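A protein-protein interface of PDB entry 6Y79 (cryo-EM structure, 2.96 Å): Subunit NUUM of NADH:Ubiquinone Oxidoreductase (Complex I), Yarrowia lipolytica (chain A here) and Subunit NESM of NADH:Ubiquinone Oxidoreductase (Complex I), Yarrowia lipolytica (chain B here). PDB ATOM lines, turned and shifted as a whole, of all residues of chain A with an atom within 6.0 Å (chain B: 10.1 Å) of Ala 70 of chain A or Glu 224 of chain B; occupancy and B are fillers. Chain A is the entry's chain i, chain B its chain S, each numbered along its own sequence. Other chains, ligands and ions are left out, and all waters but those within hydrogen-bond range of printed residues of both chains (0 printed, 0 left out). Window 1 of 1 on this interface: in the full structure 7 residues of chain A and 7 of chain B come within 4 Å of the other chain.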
ATOM      1  N   SER A  65     -14.994  19.507  -2.077  1.00  0.00           N
ATOM      2  CA  SER A  65     -14.943  18.597  -3.223  1.00  0.00           C
ATOM      3  C   SER A  65     -15.665  19.177  -4.435  1.00  0.00           C
ATOM      4  O   SER A  65     -15.138  19.150  -5.558  1.00  0.00           O
ATOM      5  CB  SER A  65     -15.547  17.254  -2.844  1.00  0.00           C
ATOM      6  OG  SER A  65     -14.792  16.608  -1.837  1.00  0.00           O
ATOM      7  N   LYS A  66     -16.858  19.734  -4.230  1.00  0.00           N
ATOM      8  CA  LYS A  66     -17.559  20.309  -5.368  1.00  0.00           C
ATOM      9  C   LYS A  66     -16.987  21.659  -5.795  1.00  0.00           C
ATOM     10  O   LYS A  66     -17.121  22.025  -6.966  1.00  0.00           O
ATOM     11  CB  LYS A  66     -19.053  20.398  -5.063  1.00  0.00           C
ATOM     12  CG  LYS A  66     -19.432  21.439  -4.063  1.00  0.00           C
ATOM     13  CD  LYS A  66     -20.788  21.162  -3.484  1.00  0.00           C
ATOM     14  CE  LYS A  66     -21.310  22.380  -2.758  1.00  0.00           C
ATOM     15  NZ  LYS A  66     -22.652  22.135  -2.177  1.00  0.00           N
ATOM     16  N   TRP A  67     -16.294  22.378  -4.906  1.00  0.00           N
ATOM     17  CA  TRP A  67     -15.605  23.593  -5.332  1.00  0.00           C
ATOM     18  C   TRP A  67     -14.372  23.261  -6.156  1.00  0.00           C
ATOM     19  O   TRP A  67     -14.050  23.974  -7.110  1.00  0.00           O
ATOM     20  CB  TRP A  67     -15.205  24.441  -4.134  1.00  0.00           C
ATOM     21  CG  TRP A  67     -16.337  25.020  -3.387  1.00  0.00           C
ATOM     22  CD1 TRP A  67     -17.630  25.098  -3.787  1.00  0.00           C
ATOM     23  CD2 TRP A  67     -16.286  25.579  -2.076  1.00  0.00           C
ATOM     24  NE1 TRP A  67     -18.392  25.684  -2.810  1.00  0.00           N
ATOM     25  CE2 TRP A  67     -17.587  25.989  -1.747  1.00  0.00           C
ATOM     26  CE3 TRP A  67     -15.262  25.780  -1.149  1.00  0.00           C
ATOM     27  CZ2 TRP A  67     -17.892  26.587  -0.533  1.00  0.00           C
ATOM     28  CZ3 TRP A  67     -15.568  26.371   0.054  1.00  0.00           C
ATOM     29  CH2 TRP A  67     -16.869  26.768   0.353  1.00  0.00           C
ATOM     30  N   ASN A  68     -13.665  22.186  -5.796  1.00  0.00           N
ATOM     31  CA  ASN A  68     -12.593  21.672  -6.641  1.00  0.00           C
ATOM     32  C   ASN A  68     -13.124  21.223  -7.998  1.00  0.00           C
ATOM     33  O   ASN A  68     -12.482  21.451  -9.032  1.00  0.00           O
ATOM     34  CB  ASN A  68     -11.909  20.511  -5.931  1.00  0.00           C
ATOM     35  CG  ASN A  68     -10.701  20.009  -6.668  1.00  0.00           C
ATOM     36  OD1 ASN A  68     -10.107  20.723  -7.457  1.00  0.00           O
ATOM     37  ND2 ASN A  68     -10.302  18.778  -6.378  1.00  0.00           N
ATOM     38  N   ALA A  69     -14.304  20.594  -8.009  1.00  0.00           N
ATOM     39  CA  ALA A  69     -14.925  20.181  -9.266  1.00  0.00           C
ATOM     40  C   ALA A  69     -15.284  21.387 -10.135  1.00  0.00           C
ATOM     41  O   ALA A  69     -15.019  21.397 -11.343  1.00  0.00           O
ATOM     42  CB  ALA A  69     -16.164  19.332  -8.974  1.00  0.00           C
ATOM     43  N   ALA A  70     -15.861  22.429  -9.530  1.00  0.00           N
ATOM     44  CA  ALA A  70     -16.215  23.633 -10.281  1.00  0.00           C
ATOM     45  C   ALA A  70     -14.992  24.430 -10.704  1.00  0.00           C
ATOM     46  O   ALA A  70     -15.039  25.157 -11.701  1.00  0.00           O
ATOM     47  CB  ALA A  70     -17.142  24.520  -9.462  1.00  0.00           C
ATOM     48  N   ALA A  71     -13.895  24.327  -9.961  1.00  0.00           N
ATOM     49  CA  ALA A  71     -12.650  24.928 -10.418  1.00  0.00           C
ATOM     50  C   ALA A  71     -12.099  24.173 -11.617  1.00  0.00           C
ATOM     51  O   ALA A  71     -11.545  24.778 -12.536  1.00  0.00           O
ATOM     52  CB  ALA A  71     -11.631  24.964  -9.283  1.00  0.00           C
ATOM     53  N   GLY A  72     -12.259  22.849 -11.633  1.00  0.00           N
ATOM     54  CA  GLY A  72     -11.961  22.093 -12.838  1.00  0.00           C
ATOM     55  C   GLY A  72     -12.857  22.429 -14.010  1.00  0.00           C
ATOM     56  O   GLY A  72     -12.428  22.366 -15.165  1.00  0.00           O
ATOM     57  N   VAL A  73     -14.101  22.807 -13.722  1.00  0.00           N
ATOM     58  CA  VAL A  73     -15.035  23.243 -14.766  1.00  0.00           C
ATOM     59  C   VAL A  73     -14.538  24.571 -15.350  1.00  0.00           C
ATOM     60  O   VAL A  73     -14.504  24.826 -16.579  1.00  0.00           O
ATOM     61  CB  VAL A  73     -16.448  23.376 -14.173  1.00  0.00           C
ATOM     62  CG1 VAL A  73     -17.347  24.184 -15.055  1.00  0.00           C
ATOM     63  CG2 VAL A  73     -16.995  21.981 -13.917  1.00  0.00           C
ATOM     64  N   TRP A  74     -14.172  25.498 -14.448  1.00  0.00           N
ATOM     65  CA  TRP A  74     -13.717  26.834 -14.920  1.00  0.00           C
ATOM     66  C   TRP A  74     -12.370  26.724 -15.608  1.00  0.00           C
ATOM     67  O   TRP A  74     -12.105  27.470 -16.533  1.00  0.00           O
ATOM     68  CB  TRP A  74     -13.779  27.797 -13.780  1.00  0.00           C
ATOM     69  CG  TRP A  74     -13.475  29.138 -14.210  1.00  0.00           C
ATOM     70  CD1 TRP A  74     -14.324  30.058 -14.733  1.00  0.00           C
ATOM     71  CD2 TRP A  74     -12.181  29.698 -14.268  1.00  0.00           C
ATOM     72  NE1 TRP A  74     -13.631  31.182 -15.082  1.00  0.00           N
ATOM     73  CE2 TRP A  74     -12.304  30.979 -14.806  1.00  0.00           C
ATOM     74  CE3 TRP A  74     -10.919  29.234 -13.902  1.00  0.00           C
ATOM     75  CZ2 TRP A  74     -11.213  31.810 -14.983  1.00  0.00           C
ATOM     76  CZ3 TRP A  74      -9.843  30.052 -14.069  1.00  0.00           C
ATOM     77  CH2 TRP A  74      -9.988  31.330 -14.610  1.00  0.00           C
ATOM     78  N   ARG A  75     -11.556  25.728 -15.225  1.00  0.00           N
ATOM     79  CA  ARG A  75     -10.332  25.453 -15.961  1.00  0.00           C
ATOM     80  C   ARG A  75     -10.570  24.664 -17.253  1.00  0.00           C
ATOM     81  O   ARG A  75      -9.708  24.735 -18.135  1.00  0.00           O
ATOM     82  CB  ARG A  75      -9.330  24.750 -15.005  1.00  0.00           C
ATOM     83  CG  ARG A  75      -7.856  24.887 -15.326  1.00  0.00           C
ATOM     84  CD  ARG A  75      -7.021  24.475 -14.107  1.00  0.00           C
ATOM     85  NE  ARG A  75      -5.743  23.865 -14.460  1.00  0.00           N
ATOM     86  CZ  ARG A  75      -4.987  23.183 -13.608  1.00  0.00           C
ATOM     87  NH1 ARG A  75      -3.838  22.654 -14.009  1.00  0.00           N
ATOM     88  NH2 ARG A  75      -5.385  23.014 -12.355  1.00  0.00           N
ATOM     89  N   ASP B 200     -25.047  37.658  -6.611  1.00  0.00           N
ATOM     90  CA  ASP B 200     -26.015  36.691  -6.093  1.00  0.00           C
ATOM     91  C   ASP B 200     -27.333  36.758  -6.852  1.00  0.00           C
ATOM     92  O   ASP B 200     -27.913  35.716  -7.191  1.00  0.00           O
ATOM     93  CB  ASP B 200     -26.249  36.944  -4.600  1.00  0.00           C
ATOM     94  CG  ASP B 200     -26.939  35.777  -3.886  1.00  0.00           C
ATOM     95  OD1 ASP B 200     -27.372  34.812  -4.551  1.00  0.00           O
ATOM     96  OD2 ASP B 200     -26.994  35.795  -2.644  1.00  0.00           O
ATOM     97  N   VAL B 203     -26.958  35.054 -10.309  1.00  0.00           N
ATOM     98  CA  VAL B 203     -26.974  33.593 -10.373  1.00  0.00           C
ATOM     99  C   VAL B 203     -28.326  33.044  -9.922  1.00  0.00           C
ATOM    100  O   VAL B 203     -28.727  31.951 -10.336  1.00  0.00           O
ATOM    101  CB  VAL B 203     -25.804  32.977  -9.591  1.00  0.00           C
ATOM    102  CG1 VAL B 203     -24.500  33.394 -10.222  1.00  0.00           C
ATOM    103  CG2 VAL B 203     -25.845  33.372  -8.146  1.00  0.00           C
ATOM    104  N   HIS B 207     -30.261  30.523 -12.556  1.00  0.00           N
ATOM    105  CA  HIS B 207     -30.572  29.204 -12.007  1.00  0.00           C
ATOM    106  C   HIS B 207     -31.514  29.365 -10.823  1.00  0.00           C
ATOM    107  O   HIS B 207     -31.068  29.467  -9.671  1.00  0.00           O
ATOM    108  CB  HIS B 207     -29.298  28.468 -11.605  1.00  0.00           C
ATOM    109  CG  HIS B 207     -28.436  28.086 -12.766  1.00  0.00           C
ATOM    110  ND1 HIS B 207     -27.131  27.669 -12.621  1.00  0.00           N
ATOM    111  CD2 HIS B 207     -28.693  28.059 -14.095  1.00  0.00           C
ATOM    112  CE1 HIS B 207     -26.619  27.405 -13.809  1.00  0.00           C
ATOM    113  NE2 HIS B 207     -27.548  27.631 -14.721  1.00  0.00           N
ATOM    114  N   GLU B 209     -33.483  27.133  -9.540  1.00  0.00           N
ATOM    115  CA  GLU B 209     -33.701  25.900  -8.787  1.00  0.00           C
ATOM    116  C   GLU B 209     -33.026  25.934  -7.416  1.00  0.00           C
ATOM    117  O   GLU B 209     -33.565  25.364  -6.453  1.00  0.00           O
ATOM    118  CB  GLU B 209     -33.227  24.705  -9.611  1.00  0.00           C
ATOM    119  CG  GLU B 209     -31.771  24.753 -10.030  1.00  0.00           C
ATOM    120  CD  GLU B 209     -30.893  23.924  -9.122  1.00  0.00           C
ATOM    121  OE1 GLU B 209     -31.447  23.143  -8.322  1.00  0.00           O
ATOM    122  OE2 GLU B 209     -29.654  24.045  -9.212  1.00  0.00           O
ATOM    123  N   ILE B 210     -31.932  26.700  -7.288  1.00  0.00           N
ATOM    124  CA  ILE B 210     -31.304  27.047  -6.010  1.00  0.00           C
ATOM    125  C   ILE B 210     -32.272  27.714  -5.039  1.00  0.00           C
ATOM    126  O   ILE B 210     -32.036  27.687  -3.823  1.00  0.00           O
ATOM    127  CB  ILE B 210     -30.083  27.960  -6.296  1.00  0.00           C
ATOM    128  CG1 ILE B 210     -29.260  27.406  -7.462  1.00  0.00           C
ATOM    129  CG2 ILE B 210     -29.165  28.136  -5.072  1.00  0.00           C
ATOM    130  CD1 ILE B 210     -27.935  28.115  -7.691  1.00  0.00           C
ATOM    131  N   ASN B 216     -28.854  27.302   4.386  1.00  0.00           N
ATOM    132  CA  ASN B 216     -27.389  27.346   4.331  1.00  0.00           C
ATOM    133  C   ASN B 216     -26.831  26.487   3.207  1.00  0.00           C
ATOM    134  O   ASN B 216     -25.643  26.605   2.882  1.00  0.00           O
ATOM    135  CB  ASN B 216     -26.764  26.918   5.662  1.00  0.00           C
ATOM    136  CG  ASN B 216     -25.495  27.711   6.003  1.00  0.00           C
ATOM    137  OD1 ASN B 216     -24.814  28.226   5.111  1.00  0.00           O
ATOM    138  ND2 ASN B 216     -25.216  27.867   7.294  1.00  0.00           N
ATOM    139  N   GLU B 217     -27.651  25.619   2.607  1.00  0.00           N
ATOM    140  CA  GLU B 217     -27.193  24.961   1.391  1.00  0.00           C
ATOM    141  C   GLU B 217     -27.158  25.953   0.237  1.00  0.00           C
ATOM    142  O   GLU B 217     -26.297  25.858  -0.650  1.00  0.00           O
ATOM    143  CB  GLU B 217     -28.075  23.755   1.073  1.00  0.00           C
ATOM    144  CG  GLU B 217     -27.823  22.556   1.987  1.00  0.00           C
ATOM    145  CD  GLU B 217     -28.672  22.561   3.236  1.00  0.00           C
ATOM    146  OE1 GLU B 217     -28.776  23.617   3.904  1.00  0.00           O
ATOM    147  OE2 GLU B 217     -29.231  21.494   3.584  1.00  0.00           O
ATOM    148  N   ARG B 218     -28.048  26.950   0.292  1.00  0.00           N
ATOM    149  CA  ARG B 218     -28.194  27.964  -0.749  1.00  0.00           C
ATOM    150  C   ARG B 218     -26.912  28.765  -0.936  1.00  0.00           C
ATOM    151  O   ARG B 218     -26.486  29.001  -2.074  1.00  0.00           O
ATOM    152  CB  ARG B 218     -29.369  28.878  -0.379  1.00  0.00           C
ATOM    153  CG  ARG B 218     -29.901  29.761  -1.474  1.00  0.00           C
ATOM    154  CD  ARG B 218     -31.181  30.454  -1.015  1.00  0.00           C
ATOM    155  NE  ARG B 218     -32.238  29.508  -0.665  1.00  0.00           N
ATOM    156  CZ  ARG B 218     -33.384  29.846  -0.082  1.00  0.00           C
ATOM    157  NH1 ARG B 218     -33.626  31.113   0.223  1.00  0.00           N
ATOM    158  NH2 ARG B 218     -34.290  28.919   0.195  1.00  0.00           N
ATOM    159  N   ASP B 219     -26.277  29.130   0.189  1.00  0.00           N
ATOM    160  CA  ASP B 219     -24.984  29.810   0.220  1.00  0.00           C
ATOM    161  C   ASP B 219     -23.942  29.101  -0.653  1.00  0.00           C
ATOM    162  O   ASP B 219     -23.433  29.671  -1.627  1.00  0.00           O
ATOM    163  CB  ASP B 219     -24.541  29.845   1.682  1.00  0.00           C
ATOM    164  CG  ASP B 219     -23.479  30.865   1.973  1.00  0.00           C
ATOM    165  OD1 ASP B 219     -23.347  31.864   1.239  1.00  0.00           O
ATOM    166  OD2 ASP B 219     -22.789  30.658   2.993  1.00  0.00           O
ATOM    167  N   ALA B 220     -23.676  27.826  -0.378  1.00  0.00           N
ATOM    168  CA  ALA B 220     -22.626  27.115  -1.099  1.00  0.00           C
ATOM    169  C   ALA B 220     -23.032  26.771  -2.524  1.00  0.00           C
ATOM    170  O   ALA B 220     -22.159  26.661  -3.390  1.00  0.00           O
ATOM    171  CB  ALA B 220     -22.234  25.848  -0.338  1.00  0.00           C
ATOM    172  N   LEU B 221     -24.333  26.599  -2.793  1.00  0.00           N
ATOM    173  CA  LEU B 221     -24.752  26.360  -4.172  1.00  0.00           C
ATOM    174  C   LEU B 221     -24.520  27.594  -5.037  1.00  0.00           C
ATOM    175  O   LEU B 221     -24.063  27.478  -6.188  1.00  0.00           O
ATOM    176  CB  LEU B 221     -26.217  25.939  -4.213  1.00  0.00           C
ATOM    177  CG  LEU B 221     -26.593  24.590  -3.599  1.00  0.00           C
ATOM    178  CD1 LEU B 221     -28.083  24.418  -3.674  1.00  0.00           C
ATOM    179  CD2 LEU B 221     -25.877  23.433  -4.272  1.00  0.00           C
ATOM    180  N   ILE B 222     -24.784  28.780  -4.475  1.00  0.00           N
ATOM    181  CA  ILE B 222     -24.452  30.040  -5.139  1.00  0.00           C
ATOM    182  C   ILE B 222     -22.956  30.122  -5.402  1.00  0.00           C
ATOM    183  O   ILE B 222     -22.528  30.491  -6.501  1.00  0.00           O
ATOM    184  CB  ILE B 222     -24.935  31.233  -4.295  1.00  0.00           C
ATOM    185  CG1 ILE B 222     -26.456  31.324  -4.294  1.00  0.00           C
ATOM    186  CG2 ILE B 222     -24.373  32.536  -4.816  1.00  0.00           C
ATOM    187  CD1 ILE B 222     -26.996  32.004  -3.058  1.00  0.00           C
ATOM    188  N   VAL B 223     -22.144  29.732  -4.410  1.00  0.00           N
ATOM    189  CA  VAL B 223     -20.685  29.834  -4.548  1.00  0.00           C
ATOM    190  C   VAL B 223     -20.164  28.908  -5.646  1.00  0.00           C
ATOM    191  O   VAL B 223     -19.310  29.303  -6.454  1.00  0.00           O
ATOM    192  CB  VAL B 223     -20.004  29.561  -3.195  1.00  0.00           C
ATOM    193  CG1 VAL B 223     -18.498  29.401  -3.349  1.00  0.00           C
ATOM    194  CG2 VAL B 223     -20.295  30.697  -2.242  1.00  0.00           C
ATOM    195  N   GLU B 224     -20.706  27.690  -5.730  1.00  0.00           N
ATOM    196  CA  GLU B 224     -20.272  26.778  -6.786  1.00  0.00           C
ATOM    197  C   GLU B 224     -20.732  27.253  -8.161  1.00  0.00           C
ATOM    198  O   GLU B 224     -20.026  27.054  -9.158  1.00  0.00           O
ATOM    199  CB  GLU B 224     -20.778  25.366  -6.513  1.00  0.00           C
ATOM    200  CG  GLU B 224     -20.154  24.337  -7.419  1.00  0.00           C
ATOM    201  CD  GLU B 224     -20.629  22.930  -7.161  1.00  0.00           C
ATOM    202  OE1 GLU B 224     -21.492  22.745  -6.280  1.00  0.00           O
ATOM    203  OE2 GLU B 224     -20.122  22.014  -7.840  1.00  0.00           O
ATOM    204  N   ARG B 225     -21.881  27.930  -8.231  1.00  0.00           N
ATOM    205  CA  ARG B 225     -22.265  28.534  -9.500  1.00  0.00           C
ATOM    206  C   ARG B 225     -21.367  29.706  -9.880  1.00  0.00           C
ATOM    207  O   ARG B 225     -21.096  29.904 -11.068  1.00  0.00           O
ATOM    208  CB  ARG B 225     -23.727  28.975  -9.459  1.00  0.00           C
ATOM    209  CG  ARG B 225     -24.701  27.818  -9.443  1.00  0.00           C
ATOM    210  CD  ARG B 225     -24.496  26.890 -10.624  1.00  0.00           C
ATOM    211  NE  ARG B 225     -25.455  25.792 -10.598  1.00  0.00           N
ATOM    212  CZ  ARG B 225     -25.473  24.792 -11.472  1.00  0.00           C
ATOM    213  NH1 ARG B 225     -24.581  24.750 -12.450  1.00  0.00           N
ATOM    214  NH2 ARG B 225     -26.386  23.835 -11.367  1.00  0.00           N
ATOM    215  N   ILE B 226     -20.890  30.475  -8.892  1.00  0.00           N
ATOM    216  CA  ILE B 226     -19.972  31.583  -9.170  1.00  0.00           C
ATOM    217  C   ILE B 226     -18.636  31.052  -9.676  1.00  0.00           C
ATOM    218  O   ILE B 226     -18.023  31.621 -10.587  1.00  0.00           O
ATOM    219  CB  ILE B 226     -19.795  32.463  -7.916  1.00  0.00           C
ATOM    220  CG1 ILE B 226     -21.091  33.167  -7.554  1.00  0.00           C
ATOM    221  CG2 ILE B 226     -18.759  33.544  -8.131  1.00  0.00           C
ATOM    222  CD1 ILE B 226     -21.083  33.721  -6.155  1.00  0.00           C
ATOM    223  N   ILE B 227     -18.179  29.935  -9.113  1.00  0.00           N
ATOM    224  CA  ILE B 227     -16.947  29.327  -9.602  1.00  0.00           C
ATOM    225  C   ILE B 227     -17.160  28.696 -10.978  1.00  0.00           C
ATOM    226  O   ILE B 227     -16.261  28.721 -11.827  1.00  0.00           O
ATOM    227  CB  ILE B 227     -16.429  28.323  -8.555  1.00  0.00           C
ATOM    228  CG1 ILE B 227     -16.153  29.051  -7.245  1.00  0.00           C
ATOM    229  CG2 ILE B 227     -15.150  27.651  -8.997  1.00  0.00           C
ATOM    230  CD1 ILE B 227     -15.912  28.141  -6.087  1.00  0.00           C
ATOM    231  N   ALA B 228     -18.360  28.188 -11.251  1.00  0.00           N
ATOM    232  CA  ALA B 228     -18.612  27.505 -12.512  1.00  0.00           C
ATOM    233  C   ALA B 228     -18.826  28.441 -13.697  1.00  0.00           C
ATOM    234  O   ALA B 228     -18.864  27.958 -14.832  1.00  0.00           O
ATOM    235  CB  ALA B 228     -19.830  26.588 -12.377  1.00  0.00           C
ATOM    236  N   GLY B 229     -18.960  29.750 -13.489  1.00  0.00           N
ATOM    237  CA  GLY B 229     -19.342  30.620 -14.586  1.00  0.00           C
ATOM    238  C   GLY B 229     -18.879  32.045 -14.407  1.00  0.00           C
ATOM    239  O   GLY B 229     -18.645  32.506 -13.285  1.00  0.00           O
ATOM    240  N   ASP B 230     -18.778  32.759 -15.536  1.00  0.00           N
ATOM    241  CA  ASP B 230     -18.340  34.151 -15.546  1.00  0.00           C
ATOM    242  C   ASP B 230     -19.337  35.074 -14.856  1.00  0.00           C
ATOM    243  O   ASP B 230     -18.989  35.726 -13.868  1.00  0.00           O
ATOM    244  CB  ASP B 230     -18.140  34.625 -16.983  1.00  0.00           C
ATOM    245  CG  ASP B 230     -17.023  33.907 -17.689  1.00  0.00           C
ATOM    246  OD1 ASP B 230     -16.315  33.093 -17.056  1.00  0.00           O
ATOM    247  OD2 ASP B 230     -16.852  34.172 -18.892  1.00  0.00           O
ATOM    248  N   TYR B 231     -20.551  35.174 -15.408  1.00  0.00           N
ATOM    249  CA  TYR B 231     -21.651  36.020 -14.913  1.00  0.00           C
ATOM    250  C   TYR B 231     -21.320  37.505 -14.915  1.00  0.00           C
ATOM    251  O   TYR B 231     -21.922  38.283 -14.177  1.00  0.00           O
ATOM    252  CB  TYR B 231     -22.113  35.610 -13.517  1.00  0.00           C
ATOM    253  CG  TYR B 231     -22.773  34.275 -13.506  1.00  0.00           C
ATOM    254  CD1 TYR B 231     -24.096  34.144 -13.893  1.00  0.00           C
ATOM    255  CD2 TYR B 231     -22.074  33.135 -13.143  1.00  0.00           C
ATOM    256  CE1 TYR B 231     -24.707  32.920 -13.909  1.00  0.00           C
ATOM    257  CE2 TYR B 231     -22.675  31.907 -13.155  1.00  0.00           C
ATOM    258  CZ  TYR B 231     -23.993  31.802 -13.537  1.00  0.00           C
ATOM    259  OH  TYR B 231     -24.600  30.567 -13.549  1.00  0.00           O
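OE2 of Glu 224 of chain B lies close to O of Lys 66 of chain A.
Ser 65 of chain A touches none of the printed residues of chain B.
Printed residues of chain B within 4 Å of Lys 66 of chain A: Glu 224 (3.1 Å).
No residue of chain B comes within 4 Å of Ala 69 of chain A.
Ala 70 of chain A touches two residues of chain B.
No residue of chain B comes within 4 Å of Gly 72 of chain A.
No residue of chain B comes within 4 Å of Val 73 of chain A.
Printed residues of chain B within 4 Å of Trp 74 of chain A: Ile 227 and Asp 230.
Of the printed residues of chain A, Val 223 of chain B touches Trp 67 (3.8 Å).
Printed residues of chain A within 4 Å of Glu 224 of chain B: Lys 66 (3.1 Å) and Ala 70 (3.6 Å).
Printed residues of chain A within 4 Å of Ile 227 of chain B: Ala 70 (3.6 Å), Ala 71 (3.7 Å) and Trp 74 (3.3 Å).
Ala 228 of chain B touches none of the printed residues of chain A.
The nearest residue of chain B that does not touch Ala 70 of chain A is Ala 228 of chain B (4.3 Å).
The nearest residue of chain A that does not touch Glu 224 of chain B is Trp 67 of chain A (4.2 Å).
Of the 11 printed residues of chain A, 5 touch a printed residue of chain B.
Among the printed residues, 8 pairs touch across the chains.
Among the printed residues, no Asp or Glu carboxylate lies within 4 Å of a Lys or Arg side-chain nitrogen of the other chain.
Among the printed residues, merely in contact across the chains: Trp 74 of chain A with Ile 227 of chain B (3.3 Å), Ala 70 of chain A with Glu 224 of chain B (3.6 Å), Ala 70 of chain A with Ile 227 of chain B (3.6 Å), Ala 71 of chain A with Ile 227 of chain B (3.7 Å), Trp 67 of chain A with Val 223 of chain B (3.8 Å), Trp 74 of chain A with Asp 230 of chain B (3.8 Å) and Trp 67 of chain A with Ala 220 of chain B (3.9 Å).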
